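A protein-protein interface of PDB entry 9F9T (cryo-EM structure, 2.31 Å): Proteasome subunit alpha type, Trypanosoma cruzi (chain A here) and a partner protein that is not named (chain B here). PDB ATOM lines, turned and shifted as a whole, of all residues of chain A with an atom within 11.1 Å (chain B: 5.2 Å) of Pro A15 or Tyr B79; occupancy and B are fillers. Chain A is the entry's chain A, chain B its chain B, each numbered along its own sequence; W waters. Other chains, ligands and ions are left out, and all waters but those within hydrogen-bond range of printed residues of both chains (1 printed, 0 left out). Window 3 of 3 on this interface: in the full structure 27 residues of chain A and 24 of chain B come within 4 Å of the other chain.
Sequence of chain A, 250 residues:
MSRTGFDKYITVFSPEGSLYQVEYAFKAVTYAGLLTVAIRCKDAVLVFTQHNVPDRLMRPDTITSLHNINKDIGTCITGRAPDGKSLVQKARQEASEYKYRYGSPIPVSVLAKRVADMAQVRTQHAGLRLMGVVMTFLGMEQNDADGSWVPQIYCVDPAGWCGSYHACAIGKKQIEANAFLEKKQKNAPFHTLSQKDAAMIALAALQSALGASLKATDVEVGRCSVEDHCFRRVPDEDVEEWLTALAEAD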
ATOM      1  N   PHE A   6      23.749  -6.648  10.821  1.00  0.00           N
ATOM      2  CA  PHE A   6      22.261  -6.543  10.761  1.00  0.00           C
ATOM      3  C   PHE A   6      21.832  -5.223  10.107  1.00  0.00           C
ATOM      4  O   PHE A   6      20.692  -5.085   9.663  1.00  0.00           O
ATOM      5  CB  PHE A   6      21.680  -6.698  12.172  1.00  0.00           C
ATOM      6  CG  PHE A   6      20.213  -7.058  12.263  1.00  0.00           C
ATOM      7  CD1 PHE A   6      19.819  -8.356  12.571  1.00  0.00           C
ATOM      8  CD2 PHE A   6      19.225  -6.091  12.110  1.00  0.00           C
ATOM      9  CE1 PHE A   6      18.476  -8.684  12.687  1.00  0.00           C
ATOM     10  CE2 PHE A   6      17.881  -6.419  12.230  1.00  0.00           C
ATOM     11  CZ  PHE A   6      17.510  -7.714  12.522  1.00  0.00           C
ATOM     12  N   ASP A   7      22.764  -4.254  10.077  1.00  0.00           N
ATOM     13  CA  ASP A   7      22.607  -2.951   9.443  1.00  0.00           C
ATOM     14  C   ASP A   7      23.215  -2.993   8.044  1.00  0.00           C
ATOM     15  O   ASP A   7      23.053  -2.054   7.258  1.00  0.00           O
ATOM     16  CB  ASP A   7      23.309  -1.855  10.253  1.00  0.00           C
ATOM     17  CG  ASP A   7      24.694  -2.235  10.775  1.00  0.00           C
ATOM     18  OD1 ASP A   7      24.940  -3.444  10.977  1.00  0.00           O
ATOM     19  OD2 ASP A   7      25.526  -1.326  10.982  1.00  0.00           O
ATOM     20  N   LYS A   8      23.933  -4.080   7.739  1.00  0.00           N
ATOM     21  CA  LYS A   8      24.586  -4.186   6.449  1.00  0.00           C
ATOM     22  C   LYS A   8      23.583  -4.671   5.418  1.00  0.00           C
ATOM     23  O   LYS A   8      23.826  -4.541   4.236  1.00  0.00           O
ATOM     24  CB  LYS A   8      25.845  -5.048   6.534  1.00  0.00           C
ATOM     25  CG  LYS A   8      27.022  -4.364   7.220  1.00  0.00           C
ATOM     26  CD  LYS A   8      28.333  -5.095   6.964  1.00  0.00           C
ATOM     27  CE  LYS A   8      29.561  -4.357   7.465  1.00  0.00           C
ATOM     28  NZ  LYS A   8      29.615  -4.299   8.945  1.00  0.00           N
ATOM     29  N   TYR A   9      22.422  -5.133   5.877  1.00  0.00           N
ATOM     30  CA  TYR A   9      21.457  -5.777   5.012  1.00  0.00           C
ATOM     31  C   TYR A   9      20.158  -4.966   4.873  1.00  0.00           C
ATOM     32  O   TYR A   9      19.375  -5.294   3.992  1.00  0.00           O
ATOM     33  CB  TYR A   9      21.328  -7.212   5.553  1.00  0.00           C
ATOM     34  CG  TYR A   9      22.644  -7.961   5.786  1.00  0.00           C
ATOM     35  CD1 TYR A   9      23.669  -7.945   4.832  1.00  0.00           C
ATOM     36  CD2 TYR A   9      22.877  -8.699   6.950  1.00  0.00           C
ATOM     37  CE1 TYR A   9      24.881  -8.605   5.027  1.00  0.00           C
ATOM     38  CE2 TYR A   9      24.083  -9.374   7.155  1.00  0.00           C
ATOM     39  CZ  TYR A   9      25.087  -9.330   6.191  1.00  0.00           C
ATOM     40  OH  TYR A   9      26.288  -9.969   6.355  1.00  0.00           O
ATOM     41  N   ILE A  10      19.896  -3.904   5.662  1.00  0.00           N
ATOM     42  CA  ILE A  10      18.699  -3.083   5.428  1.00  0.00           C
ATOM     43  C   ILE A  10      18.943  -1.595   5.723  1.00  0.00           C
ATOM     44  O   ILE A  10      20.047  -1.196   6.078  1.00  0.00           O
ATOM     45  CB  ILE A  10      17.461  -3.611   6.197  1.00  0.00           C
ATOM     46  CG1 ILE A  10      17.726  -3.804   7.695  1.00  0.00           C
ATOM     47  CG2 ILE A  10      16.891  -4.869   5.539  1.00  0.00           C
ATOM     48  CD1 ILE A  10      16.463  -3.984   8.518  1.00  0.00           C
ATOM     49  N   THR A  11      17.892  -0.783   5.528  1.00  0.00           N
ATOM     50  CA  THR A  11      17.894   0.661   5.756  1.00  0.00           C
ATOM     51  C   THR A  11      17.736   1.026   7.233  1.00  0.00           C
ATOM     52  O   THR A  11      16.696   1.510   7.686  1.00  0.00           O
ATOM     53  CB  THR A  11      16.750   1.353   5.007  1.00  0.00           C
ATOM     54  OG1 THR A  11      15.501   0.932   5.584  1.00  0.00           O
ATOM     55  CG2 THR A  11      16.863   1.115   3.508  1.00  0.00           C
ATOM     56  N   VAL A  12      18.805   0.754   7.971  1.00  0.00           N
ATOM     57  CA  VAL A  12      18.913   1.193   9.338  1.00  0.00           C
ATOM     58  C   VAL A  12      20.273   1.848   9.433  1.00  0.00           C
ATOM     59  O   VAL A  12      21.142   1.602   8.600  1.00  0.00           O
ATOM     60  CB  VAL A  12      18.719   0.065  10.390  1.00  0.00           C
ATOM     61  CG1 VAL A  12      17.289  -0.458  10.408  1.00  0.00           C
ATOM     62  CG2 VAL A  12      19.679  -1.090  10.234  1.00  0.00           C
ATOM     63  N   PHE A  13      20.386   2.711  10.445  1.00  0.00           N
ATOM     64  CA  PHE A  13      21.629   3.387  10.743  1.00  0.00           C
ATOM     65  C   PHE A  13      22.519   2.385  11.427  1.00  0.00           C
ATOM     66  O   PHE A  13      22.014   1.655  12.270  1.00  0.00           O
ATOM     67  CB  PHE A  13      21.399   4.575  11.666  1.00  0.00           C
ATOM     68  CG  PHE A  13      20.713   5.724  11.006  1.00  0.00           C
ATOM     69  CD1 PHE A  13      21.400   6.557  10.161  1.00  0.00           C
ATOM     70  CD2 PHE A  13      19.400   5.997  11.268  1.00  0.00           C
ATOM     71  CE1 PHE A  13      20.785   7.645   9.557  1.00  0.00           C
ATOM     72  CE2 PHE A  13      18.783   7.090  10.672  1.00  0.00           C
ATOM     73  CZ  PHE A  13      19.483   7.914   9.810  1.00  0.00           C
ATOM     74  N   SER A  14      23.777   2.374  11.001  1.00  0.00           N
ATOM     75  CA  SER A  14      24.892   1.877  11.787  1.00  0.00           C
ATOM     76  C   SER A  14      25.052   2.689  13.068  1.00  0.00           C
ATOM     77  O   SER A  14      24.403   3.715  13.234  1.00  0.00           O
ATOM     78  CB  SER A  14      26.189   1.966  10.979  1.00  0.00           C
ATOM     79  OG  SER A  14      26.576   3.323  10.807  1.00  0.00           O
ATOM     80  N   PRO A  15      25.936   2.293  14.006  1.00  0.00           N
ATOM     81  CA  PRO A  15      26.258   3.139  15.166  1.00  0.00           C
ATOM     82  C   PRO A  15      27.030   4.441  14.946  1.00  0.00           C
ATOM     83  O   PRO A  15      27.080   5.251  15.874  1.00  0.00           O
ATOM     84  CB  PRO A  15      27.084   2.188  16.048  1.00  0.00           C
ATOM     85  CG  PRO A  15      26.556   0.822  15.647  1.00  0.00           C
ATOM     86  CD  PRO A  15      26.464   0.930  14.138  1.00  0.00           C
ATOM     87  N   GLU A  16      27.580   4.666  13.736  1.00  0.00           N
ATOM     88  CA  GLU A  16      28.207   5.940  13.364  1.00  0.00           C
ATOM     89  C   GLU A  16      27.282   6.805  12.491  1.00  0.00           C
ATOM     90  O   GLU A  16      27.713   7.769  11.856  1.00  0.00           O
ATOM     91  CB  GLU A  16      29.514   5.673  12.628  1.00  0.00           C
ATOM     92  CG  GLU A  16      30.362   4.614  13.325  1.00  0.00           C
ATOM     93  CD  GLU A  16      31.408   3.936  12.450  1.00  0.00           C
ATOM     94  OE1 GLU A  16      31.234   3.906  11.209  1.00  0.00           O
ATOM     95  OE2 GLU A  16      32.416   3.456  13.014  1.00  0.00           O
ATOM     96  N   GLY A  17      25.987   6.460  12.446  1.00  0.00           N
ATOM     97  CA  GLY A  17      24.991   7.263  11.764  1.00  0.00           C
ATOM     98  C   GLY A  17      25.084   7.168  10.236  1.00  0.00           C
ATOM     99  O   GLY A  17      24.537   8.023   9.546  1.00  0.00           O
ATOM    100  N   SER A  18      25.749   6.131   9.725  1.00  0.00           N
ATOM    101  CA  SER A  18      25.944   5.925   8.294  1.00  0.00           C
ATOM    102  C   SER A  18      24.950   4.873   7.773  1.00  0.00           C
ATOM    103  O   SER A  18      24.500   4.026   8.532  1.00  0.00           O
ATOM    104  CB  SER A  18      27.407   5.573   8.031  1.00  0.00           C
ATOM    105  OG  SER A  18      27.694   4.232   8.399  1.00  0.00           O
ATOM    106  N   LEU A  19      24.575   4.938   6.496  1.00  0.00           N
ATOM    107  CA  LEU A  19      23.655   3.972   5.897  1.00  0.00           C
ATOM    108  C   LEU A  19      24.445   3.073   4.968  1.00  0.00           C
ATOM    109  O   LEU A  19      24.957   3.579   3.993  1.00  0.00           O
ATOM    110  CB  LEU A  19      22.568   4.713   5.091  1.00  0.00           C
ATOM    111  CG  LEU A  19      21.678   5.659   5.899  1.00  0.00           C
ATOM    112  CD1 LEU A  19      20.729   6.511   5.036  1.00  0.00           C
ATOM    113  CD2 LEU A  19      20.872   4.872   6.918  1.00  0.00           C
ATOM    114  N   TYR A  20      24.524   1.769   5.223  1.00  0.00           N
ATOM    115  CA  TYR A  20      25.489   0.935   4.498  1.00  0.00           C
ATOM    116  C   TYR A  20      25.062   0.627   3.051  1.00  0.00           C
ATOM    117  O   TYR A  20      25.891   0.561   2.169  1.00  0.00           O
ATOM    118  CB  TYR A  20      25.766  -0.312   5.344  1.00  0.00           C
ATOM    119  CG  TYR A  20      26.910  -0.104   6.328  1.00  0.00           C
ATOM    120  CD1 TYR A  20      28.143   0.358   5.883  1.00  0.00           C
ATOM    121  CD2 TYR A  20      26.749  -0.333   7.703  1.00  0.00           C
ATOM    122  CE1 TYR A  20      29.196   0.572   6.763  1.00  0.00           C
ATOM    123  CE2 TYR A  20      27.801  -0.134   8.587  1.00  0.00           C
ATOM    124  CZ  TYR A  20      29.023   0.326   8.114  1.00  0.00           C
ATOM    125  OH  TYR A  20      30.071   0.559   8.951  1.00  0.00           O
ATOM    126  N   GLU A  23      26.095   3.343   0.888  1.00  0.00           N
ATOM    127  CA  GLU A  23      27.484   3.309   0.483  1.00  0.00           C
ATOM    128  C   GLU A  23      27.749   2.240  -0.556  1.00  0.00           C
ATOM    129  O   GLU A  23      28.657   2.384  -1.347  1.00  0.00           O
ATOM    130  CB  GLU A  23      28.410   3.027   1.648  1.00  0.00           C
ATOM    131  CG  GLU A  23      28.383   4.118   2.715  1.00  0.00           C
ATOM    132  CD  GLU A  23      29.380   3.846   3.841  1.00  0.00           C
ATOM    133  OE1 GLU A  23      30.160   2.840   3.729  1.00  0.00           O
ATOM    134  OE2 GLU A  23      29.368   4.610   4.842  1.00  0.00           O
ATOM    135  N   VAL B  75      17.890   2.445  20.308  1.00  0.00           N
ATOM    136  CA  VAL B  75      19.187   2.775  19.730  1.00  0.00           C
ATOM    137  C   VAL B  75      19.069   3.374  18.316  1.00  0.00           C
ATOM    138  O   VAL B  75      19.942   4.138  17.904  1.00  0.00           O
ATOM    139  CB  VAL B  75      20.186   1.589  19.677  1.00  0.00           C
ATOM    140  CG1 VAL B  75      20.322   0.835  20.993  1.00  0.00           C
ATOM    141  CG2 VAL B  75      19.866   0.616  18.551  1.00  0.00           C
ATOM    142  N   GLN B  76      18.093   2.967  17.498  1.00  0.00           N
ATOM    143  CA  GLN B  76      18.065   3.525  16.153  1.00  0.00           C
ATOM    144  C   GLN B  76      17.867   5.056  16.225  1.00  0.00           C
ATOM    145  O   GLN B  76      18.359   5.807  15.383  1.00  0.00           O
ATOM    146  CB  GLN B  76      16.965   2.864  15.321  1.00  0.00           C
ATOM    147  CG  GLN B  76      17.448   1.621  14.618  1.00  0.00           C
ATOM    148  CD  GLN B  76      18.604   1.850  13.678  1.00  0.00           C
ATOM    149  OE1 GLN B  76      18.543   2.671  12.770  1.00  0.00           O
ATOM    150  NE2 GLN B  76      19.662   1.082  13.873  1.00  0.00           N
ATOM    151  N   ILE B  77      17.147   5.512  17.253  1.00  0.00           N
ATOM    152  CA  ILE B  77      16.975   6.928  17.483  1.00  0.00           C
ATOM    153  C   ILE B  77      18.259   7.574  17.956  1.00  0.00           C
ATOM    154  O   ILE B  77      18.391   8.770  17.732  1.00  0.00           O
ATOM    155  CB  ILE B  77      15.841   7.233  18.479  1.00  0.00           C
ATOM    156  CG1 ILE B  77      14.492   6.833  17.898  1.00  0.00           C
ATOM    157  CG2 ILE B  77      15.864   8.711  18.846  1.00  0.00           C
ATOM    158  CD1 ILE B  77      13.336   7.025  18.882  1.00  0.00           C
ATOM    159  N   GLU B  78      19.160   6.847  18.621  1.00  0.00           N
ATOM    160  CA  GLU B  78      20.438   7.443  18.994  1.00  0.00           C
ATOM    161  C   GLU B  78      21.426   7.423  17.828  1.00  0.00           C
ATOM    162  O   GLU B  78      22.312   8.262  17.723  1.00  0.00           O
ATOM    163  CB  GLU B  78      21.110   6.719  20.159  1.00  0.00           C
ATOM    164  CG  GLU B  78      20.327   6.757  21.469  1.00  0.00           C
ATOM    165  CD  GLU B  78      20.926   5.912  22.605  1.00  0.00           C
ATOM    166  OE1 GLU B  78      20.406   5.992  23.767  1.00  0.00           O
ATOM    167  OE2 GLU B  78      21.921   5.168  22.350  1.00  0.00           O
ATOM    168  N   TYR B  79      21.352   6.444  16.950  1.00  0.00           N
ATOM    169  CA  TYR B  79      22.249   6.492  15.806  1.00  0.00           C
ATOM    170  C   TYR B  79      21.822   7.603  14.851  1.00  0.00           C
ATOM    171  O   TYR B  79      22.648   8.334  14.350  1.00  0.00           O
ATOM    172  CB  TYR B  79      22.331   5.138  15.105  1.00  0.00           C
ATOM    173  CG  TYR B  79      22.690   3.950  15.993  1.00  0.00           C
ATOM    174  CD1 TYR B  79      23.377   4.092  17.194  1.00  0.00           C
ATOM    175  CD2 TYR B  79      22.307   2.662  15.610  1.00  0.00           C
ATOM    176  CE1 TYR B  79      23.687   2.990  17.984  1.00  0.00           C
ATOM    177  CE2 TYR B  79      22.624   1.556  16.383  1.00  0.00           C
ATOM    178  CZ  TYR B  79      23.302   1.719  17.583  1.00  0.00           C
ATOM    179  OH  TYR B  79      23.577   0.593  18.303  1.00  0.00           O
ATOM    180  N   ALA B  80      20.522   7.746  14.626  1.00  0.00           N
ATOM    181  CA  ALA B  80      20.025   8.849  13.836  1.00  0.00           C
ATOM    182  C   ALA B  80      20.506  10.179  14.411  1.00  0.00           C
ATOM    183  O   ALA B  80      20.933  11.045  13.680  1.00  0.00           O
ATOM    184  CB  ALA B  80      18.509   8.843  13.811  1.00  0.00           C
ATOM    185  N   THR B  81      20.377  10.339  15.737  1.00  0.00           N
ATOM    186  CA  THR B  81      20.836  11.528  16.428  1.00  0.00           C
ATOM    187  C   THR B  81      22.312  11.705  16.189  1.00  0.00           C
ATOM    188  O   THR B  81      22.752  12.825  16.014  1.00  0.00           O
ATOM    189  CB  THR B  81      20.570  11.504  17.944  1.00  0.00           C
ATOM    190  OG1 THR B  81      19.168  11.488  18.258  1.00  0.00           O
ATOM    191  CG2 THR B  81      21.185  12.717  18.593  1.00  0.00           C
ATOM    192  N   THR B  82      23.060  10.609  16.131  1.00  0.00           N
ATOM    193  CA  THR B  82      24.492  10.728  15.926  1.00  0.00           C
ATOM    194  C   THR B  82      24.774  11.356  14.569  1.00  0.00           C
ATOM    195  O   THR B  82      25.728  12.088  14.429  1.00  0.00           O
ATOM    196  CB  THR B  82      25.179   9.368  16.007  1.00  0.00           C
ATOM    197  OG1 THR B  82      25.064   8.941  17.372  1.00  0.00           O
ATOM    198  CG2 THR B  82      26.615   9.429  15.525  1.00  0.00           C
ATOM    199  N   ALA B  83      23.930  11.035  13.580  1.00  0.00           N
ATOM    200  CA  ALA B  83      24.112  11.446  12.198  1.00  0.00           C
ATOM    201  C   ALA B  83      23.741  12.922  12.074  1.00  0.00           C
ATOM    202  O   ALA B  83      24.344  13.646  11.281  1.00  0.00           O
ATOM    203  CB  ALA B  83      23.255  10.582  11.331  1.00  0.00           C
HETATM  204  O   HOH W   1      25.544   6.532  17.940  1.00  0.00           O
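NE2 of Gln B76 is in hydrogen-bond range of O of Phe A13 (2.9 Å).
Hydrophobic or aromatic side chains of chain B that line the printed part of chain A: Tyr B79, Ala B80 and Ala B83.
Of the 16 printed residues of chain A, 5 touch a printed residue of chain B.
Among the printed residues, 8 pairs touch across the chains.
Among the printed residues, no Asp or Glu carboxylate lies within 4 Å of a Lys or Arg side-chain nitrogen of the other chain.
Val A12 touches Gln B76 (CB to OE1, 3.5 Å).
Tyr B79 touches Phe A13 (CD2 to O, 3.5 Å).
Ala B80 touches Phe A13.
CB of Tyr B79 touches O of Ser A14, 3.1 Å away.
Pro A15 touches Tyr B79.
Gly A17 touches Tyr B79.
Ala B83 touches Gly A17 (CB to O, 3.4 Å).
The side-chain hydroxyl (OG) of Ser A14 sits close to the backbone NH (N) of Glu A16 (3.4 Å).
The side-chain hydroxyl (OG) of Ser A14 lies within hydrogen-bond range of the side-chain hydroxyl (OG) of Ser A18 (2.8 Å).
Water W1 lies within hydrogen-bond range of the side-chain hydroxyl (OG1) of Thr B82 and the backbone carbonyl oxygen (O) of Pro A15.
Of chain B, only Tyr B79 (3.6 Å) comes within 4 Å of Pro A15.
Of chain A, only Phe A13, Ser A14, Pro A15 and Gly A17 come within 4 Å of Tyr B79.
Gln B76 touches two residues of chain A.
No residue of chain A comes within 4 Å of Glu B78.
Of chain A, only Phe A13 comes within 4 Å of Ala B80.
No residue of chain A comes within 4 Å of Thr B82.
Ala B83 touches just one residue of chain A: Gly A17 (3.4 Å).
Printed residues of chain B within 4 Å of Val A12: Gln B76 (3.5 Å).
Of the printed residues of chain B, Ser A14 touches Tyr B79 (3.1 Å).
Of the printed residues of chain B, Phe A13 touches Gln B76 (2.9 Å), Tyr B79 (3.5 Å) and Ala B80 (3.6 Å).
Printed residues of chain B within 4 Å of Gly A17: Tyr B79 and Ala B83.
Tyr A20 touches none of the printed residues of chain B.
Asp A7 touches none of the printed residues of chain B.
The nearest residue of chain B that does not touch Pro A15 is Thr B82 (4.2 Å).
The nearest residue of chain A that does not touch Tyr B79 is Glu A16 (5.2 Å).
The nearest printed residue of chain B that does not touch Val A12 is Tyr B79 (6.6 Å).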
